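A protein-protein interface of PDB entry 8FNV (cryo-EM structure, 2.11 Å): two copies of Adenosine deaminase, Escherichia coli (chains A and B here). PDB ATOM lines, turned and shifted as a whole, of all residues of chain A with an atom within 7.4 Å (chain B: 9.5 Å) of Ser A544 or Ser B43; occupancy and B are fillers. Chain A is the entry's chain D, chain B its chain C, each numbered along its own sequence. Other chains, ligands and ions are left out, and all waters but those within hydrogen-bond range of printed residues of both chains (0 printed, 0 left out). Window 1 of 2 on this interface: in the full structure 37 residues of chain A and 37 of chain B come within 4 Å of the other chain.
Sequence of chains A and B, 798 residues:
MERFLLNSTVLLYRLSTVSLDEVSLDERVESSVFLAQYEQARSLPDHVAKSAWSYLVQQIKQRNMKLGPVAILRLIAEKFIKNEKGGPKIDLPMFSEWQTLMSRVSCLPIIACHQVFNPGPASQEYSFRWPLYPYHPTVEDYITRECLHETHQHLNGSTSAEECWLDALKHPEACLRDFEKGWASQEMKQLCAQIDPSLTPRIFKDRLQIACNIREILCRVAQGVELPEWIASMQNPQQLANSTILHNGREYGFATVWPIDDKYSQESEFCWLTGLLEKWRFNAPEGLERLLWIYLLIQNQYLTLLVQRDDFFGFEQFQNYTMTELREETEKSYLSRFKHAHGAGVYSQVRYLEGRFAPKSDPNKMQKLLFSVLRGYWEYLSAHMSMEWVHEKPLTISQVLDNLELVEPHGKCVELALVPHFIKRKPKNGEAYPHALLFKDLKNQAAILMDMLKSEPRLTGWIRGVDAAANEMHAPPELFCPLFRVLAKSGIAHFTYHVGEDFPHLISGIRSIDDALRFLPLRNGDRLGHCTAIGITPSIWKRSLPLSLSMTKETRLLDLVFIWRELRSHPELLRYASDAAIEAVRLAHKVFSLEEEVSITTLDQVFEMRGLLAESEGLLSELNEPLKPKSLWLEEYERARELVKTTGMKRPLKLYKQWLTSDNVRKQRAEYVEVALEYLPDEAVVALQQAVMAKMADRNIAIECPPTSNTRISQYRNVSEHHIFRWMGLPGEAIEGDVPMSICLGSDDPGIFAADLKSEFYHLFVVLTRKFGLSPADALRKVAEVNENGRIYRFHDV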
ATOM      1  N   TRP A 541     -15.263  -0.036   0.796  1.00  0.00           N
ATOM      2  CA  TRP A 541     -15.903   0.202   2.085  1.00  0.00           C
ATOM      3  C   TRP A 541     -15.446  -0.790   3.139  1.00  0.00           C
ATOM      4  O   TRP A 541     -15.504  -0.474   4.332  1.00  0.00           O
ATOM      5  CB  TRP A 541     -17.430   0.128   1.969  1.00  0.00           C
ATOM      6  CG  TRP A 541     -18.105  -0.049   3.296  1.00  0.00           C
ATOM      7  CD1 TRP A 541     -18.270   0.899   4.262  1.00  0.00           C
ATOM      8  CD2 TRP A 541     -18.686  -1.253   3.812  1.00  0.00           C
ATOM      9  NE1 TRP A 541     -18.923   0.363   5.344  1.00  0.00           N
ATOM     10  CE2 TRP A 541     -19.190  -0.956   5.092  1.00  0.00           C
ATOM     11  CE3 TRP A 541     -18.831  -2.550   3.313  1.00  0.00           C
ATOM     12  CZ2 TRP A 541     -19.829  -1.908   5.880  1.00  0.00           C
ATOM     13  CZ3 TRP A 541     -19.467  -3.493   4.099  1.00  0.00           C
ATOM     14  CH2 TRP A 541     -19.958  -3.167   5.367  1.00  0.00           C
ATOM     15  N   LYS A 542     -14.968  -1.964   2.737  1.00  0.00           N
ATOM     16  CA  LYS A 542     -14.465  -3.005   3.622  1.00  0.00           C
ATOM     17  C   LYS A 542     -12.977  -3.163   3.331  1.00  0.00           C
ATOM     18  O   LYS A 542     -12.565  -3.994   2.522  1.00  0.00           O
ATOM     19  CB  LYS A 542     -15.209  -4.311   3.412  1.00  0.00           C
ATOM     20  CG  LYS A 542     -15.497  -4.679   1.968  1.00  0.00           C
ATOM     21  CD  LYS A 542     -16.589  -5.730   1.890  1.00  0.00           C
ATOM     22  CE  LYS A 542     -16.653  -6.393   0.524  1.00  0.00           C
ATOM     23  NZ  LYS A 542     -15.358  -7.017   0.136  1.00  0.00           N
ATOM     24  N   ARG A 543     -12.171  -2.355   4.004  1.00  0.00           N
ATOM     25  CA  ARG A 543     -10.732  -2.347   3.800  1.00  0.00           C
ATOM     26  C   ARG A 543      -9.951  -2.599   5.077  1.00  0.00           C
ATOM     27  O   ARG A 543      -8.882  -3.214   5.025  1.00  0.00           O
ATOM     28  CB  ARG A 543     -10.310  -1.007   3.188  1.00  0.00           C
ATOM     29  CG  ARG A 543     -10.162  -1.059   1.680  1.00  0.00           C
ATOM     30  CD  ARG A 543      -9.505   0.192   1.160  1.00  0.00           C
ATOM     31  NE  ARG A 543      -9.595   0.327  -0.286  1.00  0.00           N
ATOM     32  CZ  ARG A 543      -9.173   1.388  -0.960  1.00  0.00           C
ATOM     33  NH1 ARG A 543      -8.662   2.440  -0.342  1.00  0.00           N
ATOM     34  NH2 ARG A 543      -9.266   1.394  -2.285  1.00  0.00           N
ATOM     35  N   SER A 544     -10.457  -2.143   6.222  1.00  0.00           N
ATOM     36  CA  SER A 544      -9.884  -2.463   7.523  1.00  0.00           C
ATOM     37  C   SER A 544     -10.966  -2.929   8.487  1.00  0.00           C
ATOM     38  O   SER A 544     -10.803  -2.825   9.707  1.00  0.00           O
ATOM     39  CB  SER A 544      -9.151  -1.259   8.106  1.00  0.00           C
ATOM     40  OG  SER A 544     -10.041  -0.174   8.282  1.00  0.00           O
ATOM     41  N   LEU A 545     -12.070  -3.441   7.959  1.00  0.00           N
ATOM     42  CA  LEU A 545     -13.224  -3.798   8.762  1.00  0.00           C
ATOM     43  C   LEU A 545     -13.186  -5.279   9.130  1.00  0.00           C
ATOM     44  O   LEU A 545     -12.714  -6.103   8.341  1.00  0.00           O
ATOM     45  CB  LEU A 545     -14.514  -3.497   7.999  1.00  0.00           C
ATOM     46  CG  LEU A 545     -15.251  -2.208   8.380  1.00  0.00           C
ATOM     47  CD1 LEU A 545     -14.411  -0.950   8.192  1.00  0.00           C
ATOM     48  CD2 LEU A 545     -16.602  -2.095   7.683  1.00  0.00           C
ATOM     49  N   PRO A 546     -13.672  -5.647  10.313  1.00  0.00           N
ATOM     50  CA  PRO A 546     -13.710  -7.066  10.677  1.00  0.00           C
ATOM     51  C   PRO A 546     -14.649  -7.841   9.768  1.00  0.00           C
ATOM     52  O   PRO A 546     -15.613  -7.301   9.221  1.00  0.00           O
ATOM     53  CB  PRO A 546     -14.210  -7.053  12.127  1.00  0.00           C
ATOM     54  CG  PRO A 546     -14.888  -5.745  12.297  1.00  0.00           C
ATOM     55  CD  PRO A 546     -14.194  -4.786  11.387  1.00  0.00           C
ATOM     56  N   LEU A 547     -14.352  -9.132   9.611  1.00  0.00           N
ATOM     57  CA  LEU A 547     -15.139  -9.968   8.712  1.00  0.00           C
ATOM     58  C   LEU A 547     -16.590 -10.091   9.158  1.00  0.00           C
ATOM     59  O   LEU A 547     -17.442 -10.474   8.349  1.00  0.00           O
ATOM     60  CB  LEU A 547     -14.508 -11.359   8.603  1.00  0.00           C
ATOM     61  CG  LEU A 547     -13.365 -11.562   7.601  1.00  0.00           C
ATOM     62  CD1 LEU A 547     -13.715 -11.059   6.203  1.00  0.00           C
ATOM     63  CD2 LEU A 547     -12.093 -10.894   8.099  1.00  0.00           C
ATOM     64  N   LEU A 677     -19.534  -9.572   6.574  1.00  0.00           N
ATOM     65  CA  LEU A 677     -19.217  -8.444   5.709  1.00  0.00           C
ATOM     66  C   LEU A 677     -19.626  -8.735   4.274  1.00  0.00           C
ATOM     67  O   LEU A 677     -20.203  -7.880   3.594  1.00  0.00           O
ATOM     68  CB  LEU A 677     -17.726  -8.146   5.808  1.00  0.00           C
ATOM     69  CG  LEU A 677     -17.257  -6.714   5.574  1.00  0.00           C
ATOM     70  CD1 LEU A 677     -17.719  -5.689   6.602  1.00  0.00           C
ATOM     71  CD2 LEU A 677     -15.753  -6.690   5.403  1.00  0.00           C
ATOM     72  N   SER A 714     -13.115   8.092   5.822  1.00  0.00           N
ATOM     73  CA  SER A 714     -12.233   7.459   6.796  1.00  0.00           C
ATOM     74  C   SER A 714     -11.463   6.321   6.136  1.00  0.00           C
ATOM     75  O   SER A 714     -10.306   6.052   6.461  1.00  0.00           O
ATOM     76  CB  SER A 714     -13.036   6.935   7.987  1.00  0.00           C
ATOM     77  OG  SER A 714     -14.114   6.117   7.561  1.00  0.00           O
ATOM     78  N   GLN A 715     -12.137   5.657   5.201  1.00  0.00           N
ATOM     79  CA  GLN A 715     -11.602   4.539   4.440  1.00  0.00           C
ATOM     80  C   GLN A 715     -10.891   4.975   3.167  1.00  0.00           C
ATOM     81  O   GLN A 715     -10.337   4.126   2.460  1.00  0.00           O
ATOM     82  CB  GLN A 715     -12.750   3.586   4.110  1.00  0.00           C
ATOM     83  CG  GLN A 715     -13.169   2.742   5.289  1.00  0.00           C
ATOM     84  CD  GLN A 715     -14.681   2.605   5.387  1.00  0.00           C
ATOM     85  OE1 GLN A 715     -15.402   3.599   5.372  1.00  0.00           O
ATOM     86  NE2 GLN A 715     -15.162   1.382   5.495  1.00  0.00           N
ATOM     87  N   ARG B   3      -9.308  -9.826  20.706  1.00  0.00           N
ATOM     88  CA  ARG B   3      -7.857  -9.689  20.791  1.00  0.00           C
ATOM     89  C   ARG B   3      -7.444  -8.544  21.706  1.00  0.00           C
ATOM     90  O   ARG B   3      -6.361  -8.589  22.301  1.00  0.00           O
ATOM     91  CB  ARG B   3      -7.270  -9.479  19.395  1.00  0.00           C
ATOM     92  CG  ARG B   3      -7.851  -8.288  18.650  1.00  0.00           C
ATOM     93  CD  ARG B   3      -7.121  -8.036  17.346  1.00  0.00           C
ATOM     94  NE  ARG B   3      -6.036  -7.074  17.507  1.00  0.00           N
ATOM     95  CZ  ARG B   3      -5.704  -6.150  16.615  1.00  0.00           C
ATOM     96  NH1 ARG B   3      -6.350  -6.027  15.466  1.00  0.00           N
ATOM     97  NH2 ARG B   3      -4.694  -5.327  16.881  1.00  0.00           N
ATOM     98  N   PHE B   4      -8.274  -7.505  21.815  1.00  0.00           N
ATOM     99  CA  PHE B   4      -7.938  -6.353  22.640  1.00  0.00           C
ATOM    100  C   PHE B   4      -8.073  -6.635  24.129  1.00  0.00           C
ATOM    101  O   PHE B   4      -7.553  -5.859  24.939  1.00  0.00           O
ATOM    102  CB  PHE B   4      -8.819  -5.164  22.256  1.00  0.00           C
ATOM    103  CG  PHE B   4      -8.692  -4.759  20.816  1.00  0.00           C
ATOM    104  CD1 PHE B   4      -7.463  -4.403  20.291  1.00  0.00           C
ATOM    105  CD2 PHE B   4      -9.799  -4.740  19.988  1.00  0.00           C
ATOM    106  CE1 PHE B   4      -7.340  -4.035  18.969  1.00  0.00           C
ATOM    107  CE2 PHE B   4      -9.682  -4.371  18.663  1.00  0.00           C
ATOM    108  CZ  PHE B   4      -8.451  -4.018  18.153  1.00  0.00           C
ATOM    109  N   ALA B  36      -7.097   0.547  23.324  1.00  0.00           N
ATOM    110  CA  ALA B  36      -6.229  -0.403  22.641  1.00  0.00           C
ATOM    111  C   ALA B  36      -6.576  -0.490  21.161  1.00  0.00           C
ATOM    112  O   ALA B  36      -5.683  -0.568  20.311  1.00  0.00           O
ATOM    113  CB  ALA B  36      -6.330  -1.774  23.306  1.00  0.00           C
ATOM    114  N   GLN B  37      -7.873  -0.490  20.833  1.00  0.00           N
ATOM    115  CA  GLN B  37      -8.268  -0.561  19.430  1.00  0.00           C
ATOM    116  C   GLN B  37      -7.871   0.703  18.677  1.00  0.00           C
ATOM    117  O   GLN B  37      -7.422   0.617  17.530  1.00  0.00           O
ATOM    118  CB  GLN B  37      -9.773  -0.831  19.314  1.00  0.00           C
ATOM    119  CG  GLN B  37     -10.661   0.395  19.215  1.00  0.00           C
ATOM    120  CD  GLN B  37     -10.883   0.846  17.786  1.00  0.00           C
ATOM    121  OE1 GLN B  37     -10.776   0.059  16.847  1.00  0.00           O
ATOM    122  NE2 GLN B  37     -11.202   2.121  17.614  1.00  0.00           N
ATOM    123  N   TYR B  38      -8.003   1.876  19.306  1.00  0.00           N
ATOM    124  CA  TYR B  38      -7.556   3.103  18.658  1.00  0.00           C
ATOM    125  C   TYR B  38      -6.053   3.079  18.421  1.00  0.00           C
ATOM    126  O   TYR B  38      -5.581   3.499  17.359  1.00  0.00           O
ATOM    127  CB  TYR B  38      -7.939   4.317  19.500  1.00  0.00           C
ATOM    128  CG  TYR B  38      -7.467   5.639  18.936  1.00  0.00           C
ATOM    129  CD1 TYR B  38      -8.285   6.392  18.105  1.00  0.00           C
ATOM    130  CD2 TYR B  38      -6.204   6.133  19.233  1.00  0.00           C
ATOM    131  CE1 TYR B  38      -7.865   7.607  17.598  1.00  0.00           C
ATOM    132  CE2 TYR B  38      -5.773   7.342  18.726  1.00  0.00           C
ATOM    133  CZ  TYR B  38      -6.606   8.073  17.909  1.00  0.00           C
ATOM    134  OH  TYR B  38      -6.178   9.277  17.401  1.00  0.00           O
ATOM    135  N   GLU B  39      -5.288   2.586  19.393  1.00  0.00           N
ATOM    136  CA  GLU B  39      -3.839   2.526  19.263  1.00  0.00           C
ATOM    137  C   GLU B  39      -3.401   1.511  18.209  1.00  0.00           C
ATOM    138  O   GLU B  39      -2.509   1.811  17.407  1.00  0.00           O
ATOM    139  CB  GLU B  39      -3.234   2.213  20.646  1.00  0.00           C
ATOM    140  CG  GLU B  39      -1.712   2.363  20.810  1.00  0.00           C
ATOM    141  CD  GLU B  39      -0.921   1.442  19.935  1.00  0.00           C
ATOM    142  OE1 GLU B  39      -0.818   0.187  20.180  1.00  0.00           O
ATOM    143  OE2 GLU B  39      -0.353   2.000  18.982  1.00  0.00           O
ATOM    144  N   GLN B  40      -4.054   0.354  18.134  1.00  0.00           N
ATOM    145  CA  GLN B  40      -3.610  -0.733  17.267  1.00  0.00           C
ATOM    146  C   GLN B  40      -4.257  -0.695  15.889  1.00  0.00           C
ATOM    147  O   GLN B  40      -3.554  -0.580  14.880  1.00  0.00           O
ATOM    148  CB  GLN B  40      -3.903  -2.073  17.951  1.00  0.00           C
ATOM    149  CG  GLN B  40      -3.076  -2.323  19.197  1.00  0.00           C
ATOM    150  CD  GLN B  40      -3.509  -3.565  19.940  1.00  0.00           C
ATOM    151  OE1 GLN B  40      -4.011  -4.513  19.341  1.00  0.00           O
ATOM    152  NE2 GLN B  40      -3.336  -3.558  21.259  1.00  0.00           N
ATOM    153  N   ALA B  41      -5.582  -0.779  15.821  1.00  0.00           N
ATOM    154  CA  ALA B  41      -6.333  -0.751  14.569  1.00  0.00           C
ATOM    155  C   ALA B  41      -7.122   0.557  14.556  1.00  0.00           C
ATOM    156  O   ALA B  41      -8.288   0.604  14.962  1.00  0.00           O
ATOM    157  CB  ALA B  41      -7.245  -1.971  14.444  1.00  0.00           C
ATOM    158  N   ARG B  42      -6.475   1.624  14.086  1.00  0.00           N
ATOM    159  CA  ARG B  42      -7.063   2.957  14.127  1.00  0.00           C
ATOM    160  C   ARG B  42      -8.213   3.132  13.143  1.00  0.00           C
ATOM    161  O   ARG B  42      -9.092   3.968  13.379  1.00  0.00           O
ATOM    162  CB  ARG B  42      -5.973   4.006  13.862  1.00  0.00           C
ATOM    163  CG  ARG B  42      -6.484   5.445  13.859  1.00  0.00           C
ATOM    164  CD  ARG B  42      -6.255   6.200  15.154  1.00  0.00           C
ATOM    165  NE  ARG B  42      -4.928   6.080  15.734  1.00  0.00           N
ATOM    166  CZ  ARG B  42      -4.001   7.023  15.682  1.00  0.00           C
ATOM    167  NH1 ARG B  42      -4.173   8.141  14.972  1.00  0.00           N
ATOM    168  NH2 ARG B  42      -2.861   6.820  16.333  1.00  0.00           N
ATOM    169  N   SER B  43      -8.250   2.354  12.067  1.00  0.00           N
ATOM    170  CA  SER B  43      -9.180   2.612  10.976  1.00  0.00           C
ATOM    171  C   SER B  43     -10.598   2.127  11.261  1.00  0.00           C
ATOM    172  O   SER B  43     -11.484   2.346  10.427  1.00  0.00           O
ATOM    173  CB  SER B  43      -8.659   1.971   9.692  1.00  0.00           C
ATOM    174  OG  SER B  43      -8.121   0.687   9.949  1.00  0.00           O
ATOM    175  N   LEU B  44     -10.844   1.486  12.399  1.00  0.00           N
ATOM    176  CA  LEU B  44     -12.211   1.112  12.750  1.00  0.00           C
ATOM    177  C   LEU B  44     -13.029   2.381  12.974  1.00  0.00           C
ATOM    178  O   LEU B  44     -12.606   3.250  13.745  1.00  0.00           O
ATOM    179  CB  LEU B  44     -12.229   0.234  14.002  1.00  0.00           C
ATOM    180  CG  LEU B  44     -12.336  -1.281  13.785  1.00  0.00           C
ATOM    181  CD1 LEU B  44     -12.452  -2.040  15.103  1.00  0.00           C
ATOM    182  CD2 LEU B  44     -13.473  -1.663  12.843  1.00  0.00           C
ATOM    183  N   PRO B  45     -14.201   2.534  12.329  1.00  0.00           N
ATOM    184  CA  PRO B  45     -14.865   3.847  12.348  1.00  0.00           C
ATOM    185  C   PRO B  45     -15.615   4.173  13.634  1.00  0.00           C
ATOM    186  O   PRO B  45     -16.725   4.714  13.587  1.00  0.00           O
ATOM    187  CB  PRO B  45     -15.837   3.758  11.161  1.00  0.00           C
ATOM    188  CG  PRO B  45     -15.446   2.538  10.395  1.00  0.00           C
ATOM    189  CD  PRO B  45     -14.876   1.614  11.402  1.00  0.00           C
ATOM    190  N   ASP B  46     -15.023   3.859  14.786  1.00  0.00           N
ATOM    191  CA  ASP B  46     -15.444   4.425  16.066  1.00  0.00           C
ATOM    192  C   ASP B  46     -16.835   3.985  16.518  1.00  0.00           C
ATOM    193  O   ASP B  46     -17.253   4.323  17.630  1.00  0.00           O
ATOM    194  CB  ASP B  46     -15.398   5.953  15.994  1.00  0.00           C
ATOM    195  CG  ASP B  46     -15.593   6.608  17.348  1.00  0.00           C
ATOM    196  OD1 ASP B  46     -15.057   6.083  18.346  1.00  0.00           O
ATOM    197  OD2 ASP B  46     -16.284   7.645  17.414  1.00  0.00           O
ATOM    198  N   HIS B  47     -17.560   3.237  15.688  1.00  0.00           N
ATOM    199  CA  HIS B  47     -18.869   2.733  16.087  1.00  0.00           C
ATOM    200  C   HIS B  47     -18.985   1.243  15.802  1.00  0.00           C
ATOM    201  O   HIS B  47     -19.723   0.529  16.490  1.00  0.00           O
ATOM    202  CB  HIS B  47     -19.991   3.496  15.379  1.00  0.00           C
ATOM    203  CG  HIS B  47     -19.925   3.427  13.885  1.00  0.00           C
ATOM    204  ND1 HIS B  47     -19.071   4.210  13.140  1.00  0.00           N
ATOM    205  CD2 HIS B  47     -20.585   2.644  13.001  1.00  0.00           C
ATOM    206  CE1 HIS B  47     -19.234   3.935  11.858  1.00  0.00           C
ATOM    207  NE2 HIS B  47     -20.144   2.985  11.747  1.00  0.00           N
ATOM    208  N   VAL B  48     -18.246   0.760  14.804  1.00  0.00           N
ATOM    209  CA  VAL B  48     -18.099  -0.681  14.636  1.00  0.00           C
ATOM    210  C   VAL B  48     -17.506  -1.283  15.903  1.00  0.00           C
ATOM    211  O   VAL B  48     -17.899  -2.371  16.336  1.00  0.00           O
ATOM    212  CB  VAL B  48     -17.237  -0.989  13.397  1.00  0.00           C
ATOM    213  CG1 VAL B  48     -16.824  -2.453  13.375  1.00  0.00           C
ATOM    214  CG2 VAL B  48     -17.986  -0.622  12.124  1.00  0.00           C
ATOM    215  N   ALA B  49     -16.562  -0.571  16.522  1.00  0.00           N
ATOM    216  CA  ALA B  49     -15.978  -1.028  17.779  1.00  0.00           C
ATOM    217  C   ALA B  49     -17.012  -1.054  18.900  1.00  0.00           C
ATOM    218  O   ALA B  49     -17.098  -2.034  19.653  1.00  0.00           O
ATOM    219  CB  ALA B  49     -14.803  -0.127  18.150  1.00  0.00           C
ATOM    220  N   THR B 100      -4.077 -13.606  11.480  1.00  0.00           N
ATOM    221  CA  THR B 100      -4.055 -12.231  11.965  1.00  0.00           C
ATOM    222  C   THR B 100      -4.150 -12.192  13.486  1.00  0.00           C
ATOM    223  O   THR B 100      -3.484 -11.380  14.138  1.00  0.00           O
ATOM    224  CB  THR B 100      -5.190 -11.422  11.336  1.00  0.00           C
ATOM    225  OG1 THR B 100      -5.135 -11.547   9.911  1.00  0.00           O
ATOM    226  CG2 THR B 100      -5.070  -9.957  11.718  1.00  0.00           C
ATOM    227  N   ARG B 717      -2.690  -4.384   2.921  1.00  0.00           N
ATOM    228  CA  ARG B 717      -3.807  -4.531   3.849  1.00  0.00           C
ATOM    229  C   ARG B 717      -4.151  -5.998   4.042  1.00  0.00           C
ATOM    230  O   ARG B 717      -4.201  -6.498   5.172  1.00  0.00           O
ATOM    231  CB  ARG B 717      -5.041  -3.796   3.330  1.00  0.00           C
ATOM    232  CG  ARG B 717      -4.875  -2.319   3.085  1.00  0.00           C
ATOM    233  CD  ARG B 717      -6.166  -1.589   3.425  1.00  0.00           C
ATOM    234  NE  ARG B 717      -6.454  -0.482   2.521  1.00  0.00           N
ATOM    235  CZ  ARG B 717      -6.562   0.792   2.882  1.00  0.00           C
ATOM    236  NH1 ARG B 717      -6.393   1.179   4.136  1.00  0.00           N
ATOM    237  NH2 ARG B 717      -6.837   1.704   1.956  1.00  0.00           N
ATOM    238  N   ASN B 718      -4.387  -6.695   2.938  1.00  0.00           N
ATOM    239  CA  ASN B 718      -4.786  -8.090   2.926  1.00  0.00           C
ATOM    240  C   ASN B 718      -3.694  -8.918   2.267  1.00  0.00           C
ATOM    241  O   ASN B 718      -2.913  -8.420   1.452  1.00  0.00           O
ATOM    242  CB  ASN B 718      -6.108  -8.273   2.175  1.00  0.00           C
ATOM    243  CG  ASN B 718      -6.195  -7.401   0.939  1.00  0.00           C
ATOM    244  OD1 ASN B 718      -5.622  -6.312   0.896  1.00  0.00           O
ATOM    245  ND2 ASN B 718      -6.900  -7.877  -0.078  1.00  0.00           N
ATOM    246  N   GLU B 721      -2.882  -9.140  -1.614  1.00  0.00           N
ATOM    247  CA  GLU B 721      -2.092  -8.138  -2.317  1.00  0.00           C
ATOM    248  C   GLU B 721      -0.603  -8.458  -2.319  1.00  0.00           C
ATOM    249  O   GLU B 721       0.182  -7.677  -2.867  1.00  0.00           O
ATOM    250  CB  GLU B 721      -2.322  -6.759  -1.692  1.00  0.00           C
ATOM    251  CG  GLU B 721      -3.697  -6.174  -1.977  1.00  0.00           C
ATOM    252  CD  GLU B 721      -3.993  -4.942  -1.145  1.00  0.00           C
ATOM    253  OE1 GLU B 721      -3.054  -4.398  -0.528  1.00  0.00           O
ATOM    254  OE2 GLU B 721      -5.165  -4.515  -1.109  1.00  0.00           O
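The side-chain hydroxyl (OG) of Ser B43 is in hydrogen-bond range of the side-chain hydroxyl (OG) of Ser A544. NH1 of Arg A543 sits close to NH2 of Arg B717 (3.0 Å).
No position is printed for both chains. Of the 4 pairs that touch across the chains among the printed residues, none has its exchanged pair printed and touching as well.
CD2 of Leu B44 touches CD of Pro A546, 3.5 Å away. Pro A546 touches Val B48.
Of the 10 printed residues of chain A, 3 touch a printed residue of chain B. Hydrophobic or aromatic side chains of chain A within 4 Å of the printed part of chain B: Pro A546. Of the 20 printed residues of chain B, 4 touch a printed residue of chain A. Hydrophobic or aromatic side chains of chain B within 4 Å of the printed part of chain A: Leu B44 and Val B48. Along chain B the printed residues that touch a printed residue of chain A span positions 43 to 717. Among the printed residues, no Asp or Glu carboxylate lies within 4 Å of a Lys or Arg side-chain nitrogen of the other chain.
Of the printed residues of chain B, Arg A543 touches Arg B717 (3.0 Å). Ser A544 touches one residue of chain B. Of the printed residues of chain B, Pro A546 touches Leu B44 (3.5 Å) and Val B48 (3.97 Å). Ser A714 touches none of the printed residues of chain B. Of the printed residues of chain A, Leu B44 touches Pro A546 (3.5 Å). Printed residues of chain A within 4 Å of Val B48: Pro A546 (3.97 Å). Of the printed residues of chain A, Arg B717 touches Arg A543 (3.0 Å). The nearest printed residue of chain A that does not touch Arg B717 is Gln A715 (4.3 Å).
The backbone NH (N) of Arg B717 is in hydrogen-bond range of the side-chain carboxylate (OE1) of Glu B721, at 3.5 Å.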
